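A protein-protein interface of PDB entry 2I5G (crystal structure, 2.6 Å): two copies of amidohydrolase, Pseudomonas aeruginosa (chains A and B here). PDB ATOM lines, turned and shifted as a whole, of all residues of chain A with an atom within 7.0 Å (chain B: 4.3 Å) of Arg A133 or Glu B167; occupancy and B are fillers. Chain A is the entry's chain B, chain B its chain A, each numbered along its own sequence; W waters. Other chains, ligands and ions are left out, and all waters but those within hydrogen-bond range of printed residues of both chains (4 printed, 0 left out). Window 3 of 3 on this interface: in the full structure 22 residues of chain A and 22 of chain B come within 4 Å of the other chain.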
ATOM      1  N   GLN A 123     -28.812  24.001  14.879  1.00  0.00           N
ATOM      2  CA  GLN A 123     -27.519  24.595  15.199  1.00  0.00           C
ATOM      3  C   GLN A 123     -27.526  25.496  16.416  1.00  0.00           C
ATOM      4  O   GLN A 123     -28.487  26.216  16.676  1.00  0.00           O
ATOM      5  CB  GLN A 123     -26.947  25.361  14.003  1.00  0.00           C
ATOM      6  CG  GLN A 123     -25.559  25.932  14.282  1.00  0.00           C
ATOM      7  CD  GLN A 123     -24.721  26.123  13.031  1.00  0.00           C
ATOM      8  OE1 GLN A 123     -24.503  25.180  12.269  1.00  0.00           O
ATOM      9  NE2 GLN A 123     -24.236  27.344  12.820  1.00  0.00           N
ATOM     10  N   THR A 128     -24.523  21.346  16.817  1.00  0.00           N
ATOM     11  CA  THR A 128     -25.712  21.134  16.009  1.00  0.00           C
ATOM     12  C   THR A 128     -26.382  19.889  16.555  1.00  0.00           C
ATOM     13  O   THR A 128     -25.712  19.000  17.082  1.00  0.00           O
ATOM     14  CB  THR A 128     -25.358  20.909  14.530  1.00  0.00           C
ATOM     15  OG1 THR A 128     -24.523  21.980  14.074  1.00  0.00           O
ATOM     16  CG2 THR A 128     -26.623  20.872  13.676  1.00  0.00           C
ATOM     17  N   GLY A 129     -27.704  19.829  16.449  1.00  0.00           N
ATOM     18  CA  GLY A 129     -28.425  18.670  16.941  1.00  0.00           C
ATOM     19  C   GLY A 129     -28.939  17.808  15.808  1.00  0.00           C
ATOM     20  O   GLY A 129     -28.827  18.189  14.645  1.00  0.00           O
ATOM     21  N   CYS A 130     -29.485  16.639  16.133  1.00  0.00           N
ATOM     22  CA  CYS A 130     -30.036  15.760  15.107  1.00  0.00           C
ATOM     23  C   CYS A 130     -31.055  16.641  14.396  1.00  0.00           C
ATOM     24  O   CYS A 130     -31.394  17.695  14.912  1.00  0.00           O
ATOM     25  CB  CYS A 130     -30.718  14.553  15.761  1.00  0.00           C
ATOM     26  SG  CYS A 130     -32.033  14.965  16.955  1.00  0.00           S
ATOM     27  N   TYR A 131     -31.530  16.242  13.226  1.00  0.00           N
ATOM     28  CA  TYR A 131     -32.515  17.045  12.478  1.00  0.00           C
ATOM     29  C   TYR A 131     -31.926  18.036  11.474  1.00  0.00           C
ATOM     30  O   TYR A 131     -32.676  18.743  10.808  1.00  0.00           O
ATOM     31  CB  TYR A 131     -33.447  17.835  13.420  1.00  0.00           C
ATOM     32  CG  TYR A 131     -34.497  17.012  14.135  1.00  0.00           C
ATOM     33  CD1 TYR A 131     -34.727  17.178  15.498  1.00  0.00           C
ATOM     34  CD2 TYR A 131     -35.267  16.075  13.448  1.00  0.00           C
ATOM     35  CE1 TYR A 131     -35.695  16.427  16.159  1.00  0.00           C
ATOM     36  CE2 TYR A 131     -36.239  15.320  14.103  1.00  0.00           C
ATOM     37  CZ  TYR A 131     -36.444  15.499  15.459  1.00  0.00           C
ATOM     38  OH  TYR A 131     -37.384  14.738  16.114  1.00  0.00           O
ATOM     39  N   GLU A 132     -30.602  18.102  11.360  1.00  0.00           N
ATOM     40  CA  GLU A 132     -29.969  19.031  10.415  1.00  0.00           C
ATOM     41  C   GLU A 132     -28.487  18.711  10.235  1.00  0.00           C
ATOM     42  O   GLU A 132     -27.846  18.217  11.155  1.00  0.00           O
ATOM     43  CB  GLU A 132     -30.171  20.484  10.906  1.00  0.00           C
ATOM     44  CG  GLU A 132     -29.170  21.523  10.410  1.00  0.00           C
ATOM     45  CD  GLU A 132     -29.577  22.968  10.755  1.00  0.00           C
ATOM     46  OE1 GLU A 132     -30.349  23.582   9.978  1.00  0.00           O
ATOM     47  OE2 GLU A 132     -29.131  23.493  11.803  1.00  0.00           O
ATOM     48  N   ARG A 133     -27.959  18.967   9.039  1.00  0.00           N
ATOM     49  CA  ARG A 133     -26.544  18.732   8.743  1.00  0.00           C
ATOM     50  C   ARG A 133     -25.708  19.120   9.968  1.00  0.00           C
ATOM     51  O   ARG A 133     -25.628  20.293  10.319  1.00  0.00           O
ATOM     52  CB  ARG A 133     -26.129  19.583   7.537  1.00  0.00           C
ATOM     53  CG  ARG A 133     -24.639  19.580   7.230  1.00  0.00           C
ATOM     54  CD  ARG A 133     -24.230  20.913   6.611  1.00  0.00           C
ATOM     55  NE  ARG A 133     -24.702  21.072   5.242  1.00  0.00           N
ATOM     56  CZ  ARG A 133     -24.815  22.241   4.619  1.00  0.00           C
ATOM     57  NH1 ARG A 133     -24.499  23.369   5.240  1.00  0.00           N
ATOM     58  NH2 ARG A 133     -25.247  22.284   3.368  1.00  0.00           N
ATOM     59  N   ASP A 134     -25.081  18.139  10.609  1.00  0.00           N
ATOM     60  CA  ASP A 134     -24.299  18.400  11.814  1.00  0.00           C
ATOM     61  C   ASP A 134     -22.848  18.823  11.593  1.00  0.00           C
ATOM     62  O   ASP A 134     -22.009  18.008  11.209  1.00  0.00           O
ATOM     63  CB  ASP A 134     -24.328  17.168  12.718  1.00  0.00           C
ATOM     64  CG  ASP A 134     -23.711  17.432  14.071  1.00  0.00           C
ATOM     65  OD1 ASP A 134     -23.626  16.494  14.892  1.00  0.00           O
ATOM     66  OD2 ASP A 134     -23.312  18.591  14.307  1.00  0.00           O
ATOM     67  N   GLY A 135     -22.556  20.092  11.875  1.00  0.00           N
ATOM     68  CA  GLY A 135     -21.207  20.614  11.701  1.00  0.00           C
ATOM     69  C   GLY A 135     -20.191  20.169  12.743  1.00  0.00           C
ATOM     70  O   GLY A 135     -18.990  20.237  12.506  1.00  0.00           O
ATOM     71  N   GLY A 136     -20.664  19.711  13.898  1.00  0.00           N
ATOM     72  CA  GLY A 136     -19.758  19.263  14.937  1.00  0.00           C
ATOM     73  C   GLY A 136     -19.724  20.203  16.125  1.00  0.00           C
ATOM     74  O   GLY A 136     -20.541  21.113  16.236  1.00  0.00           O
ATOM     75  N   GLY B 135     -19.019  24.790   9.175  1.00  0.00           N
ATOM     76  CA  GLY B 135     -20.089  23.816   9.008  1.00  0.00           C
ATOM     77  C   GLY B 135     -21.106  24.093   7.911  1.00  0.00           C
ATOM     78  O   GLY B 135     -21.957  23.252   7.625  1.00  0.00           O
ATOM     79  N   GLY B 136     -21.027  25.265   7.290  1.00  0.00           N
ATOM     80  CA  GLY B 136     -21.962  25.605   6.236  1.00  0.00           C
ATOM     81  C   GLY B 136     -23.106  26.440   6.762  1.00  0.00           C
ATOM     82  O   GLY B 136     -23.199  26.690   7.968  1.00  0.00           O
ATOM     83  N   LEU B 137     -23.975  26.874   5.856  1.00  0.00           N
ATOM     84  CA  LEU B 137     -25.137  27.683   6.211  1.00  0.00           C
ATOM     85  C   LEU B 137     -26.171  26.797   6.908  1.00  0.00           C
ATOM     86  O   LEU B 137     -26.582  25.759   6.370  1.00  0.00           O
ATOM     87  CB  LEU B 137     -25.737  28.298   4.949  1.00  0.00           C
ATOM     88  CG  LEU B 137     -26.926  29.231   5.150  1.00  0.00           C
ATOM     89  CD1 LEU B 137     -26.538  30.372   6.082  1.00  0.00           C
ATOM     90  CD2 LEU B 137     -27.375  29.763   3.803  1.00  0.00           C
ATOM     91  N   LYS B 163     -17.317  27.636   3.231  1.00  0.00           N
ATOM     92  CA  LYS B 163     -18.485  26.777   3.093  1.00  0.00           C
ATOM     93  C   LYS B 163     -19.777  27.567   3.222  1.00  0.00           C
ATOM     94  O   LYS B 163     -20.639  27.510   2.344  1.00  0.00           O
ATOM     95  CB  LYS B 163     -18.481  25.664   4.149  1.00  0.00           C
ATOM     96  CG  LYS B 163     -17.811  24.370   3.706  1.00  0.00           C
ATOM     97  CD  LYS B 163     -16.291  24.491   3.646  1.00  0.00           C
ATOM     98  CE  LYS B 163     -15.663  24.418   5.038  1.00  0.00           C
ATOM     99  NZ  LYS B 163     -15.877  23.092   5.693  1.00  0.00           N
ATOM    100  N   THR B 164     -19.931  28.306   4.312  1.00  0.00           N
ATOM    101  CA  THR B 164     -21.162  29.056   4.479  1.00  0.00           C
ATOM    102  C   THR B 164     -21.229  30.233   3.509  1.00  0.00           C
ATOM    103  O   THR B 164     -22.316  30.637   3.081  1.00  0.00           O
ATOM    104  CB  THR B 164     -21.365  29.519   5.956  1.00  0.00           C
ATOM    105  OG1 THR B 164     -21.888  30.851   5.980  1.00  0.00           O
ATOM    106  CG2 THR B 164     -20.076  29.453   6.732  1.00  0.00           C
ATOM    107  N   SER B 165     -20.074  30.770   3.135  1.00  0.00           N
ATOM    108  CA  SER B 165     -20.072  31.883   2.199  1.00  0.00           C
ATOM    109  C   SER B 165     -20.667  31.469   0.863  1.00  0.00           C
ATOM    110  O   SER B 165     -21.498  32.183   0.305  1.00  0.00           O
ATOM    111  CB  SER B 165     -18.656  32.417   1.981  1.00  0.00           C
ATOM    112  OG  SER B 165     -18.294  33.323   3.011  1.00  0.00           O
ATOM    113  N   GLU B 166     -20.256  30.312   0.350  1.00  0.00           N
ATOM    114  CA  GLU B 166     -20.763  29.853  -0.936  1.00  0.00           C
ATOM    115  C   GLU B 166     -22.263  29.594  -0.926  1.00  0.00           C
ATOM    116  O   GLU B 166     -22.955  29.913  -1.890  1.00  0.00           O
ATOM    117  CB  GLU B 166     -20.042  28.589  -1.391  1.00  0.00           C
ATOM    118  CG  GLU B 166     -20.487  28.148  -2.779  1.00  0.00           C
ATOM    119  CD  GLU B 166     -19.811  26.878  -3.249  1.00  0.00           C
ATOM    120  OE1 GLU B 166     -18.557  26.839  -3.255  1.00  0.00           O
ATOM    121  OE2 GLU B 166     -20.534  25.923  -3.618  1.00  0.00           O
ATOM    122  N   GLU B 167     -22.767  29.011   0.156  1.00  0.00           N
ATOM    123  CA  GLU B 167     -24.194  28.722   0.259  1.00  0.00           C
ATOM    124  C   GLU B 167     -24.993  30.017   0.241  1.00  0.00           C
ATOM    125  O   GLU B 167     -26.044  30.101  -0.392  1.00  0.00           O
ATOM    126  CB  GLU B 167     -24.482  27.929   1.536  1.00  0.00           C
ATOM    127  CG  GLU B 167     -23.977  26.495   1.474  1.00  0.00           C
ATOM    128  CD  GLU B 167     -24.024  25.780   2.812  1.00  0.00           C
ATOM    129  OE1 GLU B 167     -25.104  25.720   3.428  1.00  0.00           O
ATOM    130  OE2 GLU B 167     -22.976  25.266   3.250  1.00  0.00           O
ATOM    131  N   VAL B 168     -24.480  31.034   0.922  1.00  0.00           N
ATOM    132  CA  VAL B 168     -25.150  32.328   0.967  1.00  0.00           C
ATOM    133  C   VAL B 168     -25.216  32.969  -0.425  1.00  0.00           C
ATOM    134  O   VAL B 168     -26.232  33.553  -0.800  1.00  0.00           O
ATOM    135  CB  VAL B 168     -24.429  33.292   1.957  1.00  0.00           C
ATOM    136  CG1 VAL B 168     -25.032  34.695   1.876  1.00  0.00           C
ATOM    137  CG2 VAL B 168     -24.551  32.753   3.373  1.00  0.00           C
ATOM    138  N   ILE B 169     -24.140  32.860  -1.195  1.00  0.00           N
ATOM    139  CA  ILE B 169     -24.135  33.444  -2.532  1.00  0.00           C
ATOM    140  C   ILE B 169     -25.176  32.759  -3.417  1.00  0.00           C
ATOM    141  O   ILE B 169     -25.840  33.401  -4.236  1.00  0.00           O
ATOM    142  CB  ILE B 169     -22.750  33.305  -3.210  1.00  0.00           C
ATOM    143  CG1 ILE B 169     -21.687  34.036  -2.381  1.00  0.00           C
ATOM    144  CG2 ILE B 169     -22.811  33.864  -4.636  1.00  0.00           C
ATOM    145  CD1 ILE B 169     -20.276  33.846  -2.882  1.00  0.00           C
ATOM    146  N   LEU B 170     -25.310  31.450  -3.237  1.00  0.00           N
ATOM    147  CA  LEU B 170     -26.243  30.643  -4.011  1.00  0.00           C
ATOM    148  C   LEU B 170     -27.694  30.781  -3.550  1.00  0.00           C
ATOM    149  O   LEU B 170     -28.616  30.510  -4.309  1.00  0.00           O
ATOM    150  CB  LEU B 170     -25.814  29.176  -3.923  1.00  0.00           C
ATOM    151  CG  LEU B 170     -25.141  28.462  -5.103  1.00  0.00           C
ATOM    152  CD1 LEU B 170     -24.389  29.435  -5.992  1.00  0.00           C
ATOM    153  CD2 LEU B 170     -24.212  27.395  -4.545  1.00  0.00           C
ATOM    154  N   GLU B 171     -27.890  31.210  -2.307  1.00  0.00           N
ATOM    155  CA  GLU B 171     -29.226  31.349  -1.728  1.00  0.00           C
ATOM    156  C   GLU B 171     -29.883  32.721  -1.885  1.00  0.00           C
ATOM    157  O   GLU B 171     -31.092  32.808  -2.096  1.00  0.00           O
ATOM    158  CB  GLU B 171     -29.164  30.960  -0.242  1.00  0.00           C
ATOM    159  CG  GLU B 171     -30.349  31.383   0.630  1.00  0.00           C
ATOM    160  CD  GLU B 171     -31.583  30.525   0.432  1.00  0.00           C
ATOM    161  OE1 GLU B 171     -31.466  29.282   0.477  1.00  0.00           O
ATOM    162  OE2 GLU B 171     -32.677  31.099   0.247  1.00  0.00           O
HETATM  163  O   HOH W   1     -25.562  23.206   8.118  1.00  0.00           O
HETATM  164  O   HOH W   2     -21.988  26.571  10.524  1.00  0.00           O
HETATM  165  O   HOH W   3     -22.643  21.450   9.256  1.00  0.00           O
HETATM  166  O   HOH W   4     -28.488  23.142   7.237  1.00  0.00           O
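The side-chain carboxylate (OE1) of Glu B167 is in salt-bridge range of the guanidinium group (NH1) of Arg A133, 3.0 Å away.
The guanidinium group (NH1) of Arg A133 is in hydrogen-bond range of the backbone carbonyl oxygen (O) of Leu B137 (3.4 Å).
O of Gly B135 lies close to NH1 of Arg A133 (3.5 Å).
The backbone NH (N) of Leu B137 is in hydrogen-bond range of the side-chain carboxylate (OE1) of Glu B167, 2.9 Å away.
NH1 of Arg A133 touches CA of Gly B136 (3.5 Å).
Printed residues of chain B within 4 Å of Arg A133: Gly B135, Gly B136, Leu B137 and Glu B167.
Of chain A, only Arg A133 comes within 4 Å of Glu B167.
Of the printed residues of chain A, Gly B136 touches Arg A133.
Of the printed residues of chain A, Gly B135 touches Arg A133.
Tyr A131 touches none of the printed residues of chain B.
The nearest printed residue of chain B that does not touch Arg A133 is Lys B163 (6.4 Å).
The nearest printed residue of chain A that does not touch Leu B137 is Glu A132 (5.7 Å).
Of the 10 printed residues of chain A, 1 touches a printed residue of chain B.
Along chain B the printed residues that touch a printed residue of chain A span positions 135 to 167.
Positions printed for both chains: 135 and 136.
Of the 4 pairs that touch across the chains among the printed residues, none has its exchanged pair printed and touching as well.
Water W3 lies within hydrogen-bond range of O of Gly B135 (2.5 Å), N of Gly A135 (3.0 Å) and O of Arg A133 (3.4 Å).
Water W2 lies within hydrogen-bond range of O of Gly B136 (2.8 Å) and NE2 of Gln A123 (3.3 Å).
Water W1 lies within hydrogen-bond range of the guanidinium group of Arg A133 and the backbone carbonyl oxygen of Leu B137.
Water W4 bridges the side-chain carboxylate of Glu A132 (3.3 Å) and the backbone carbonyl oxygen of Leu B137 (3.4 Å).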
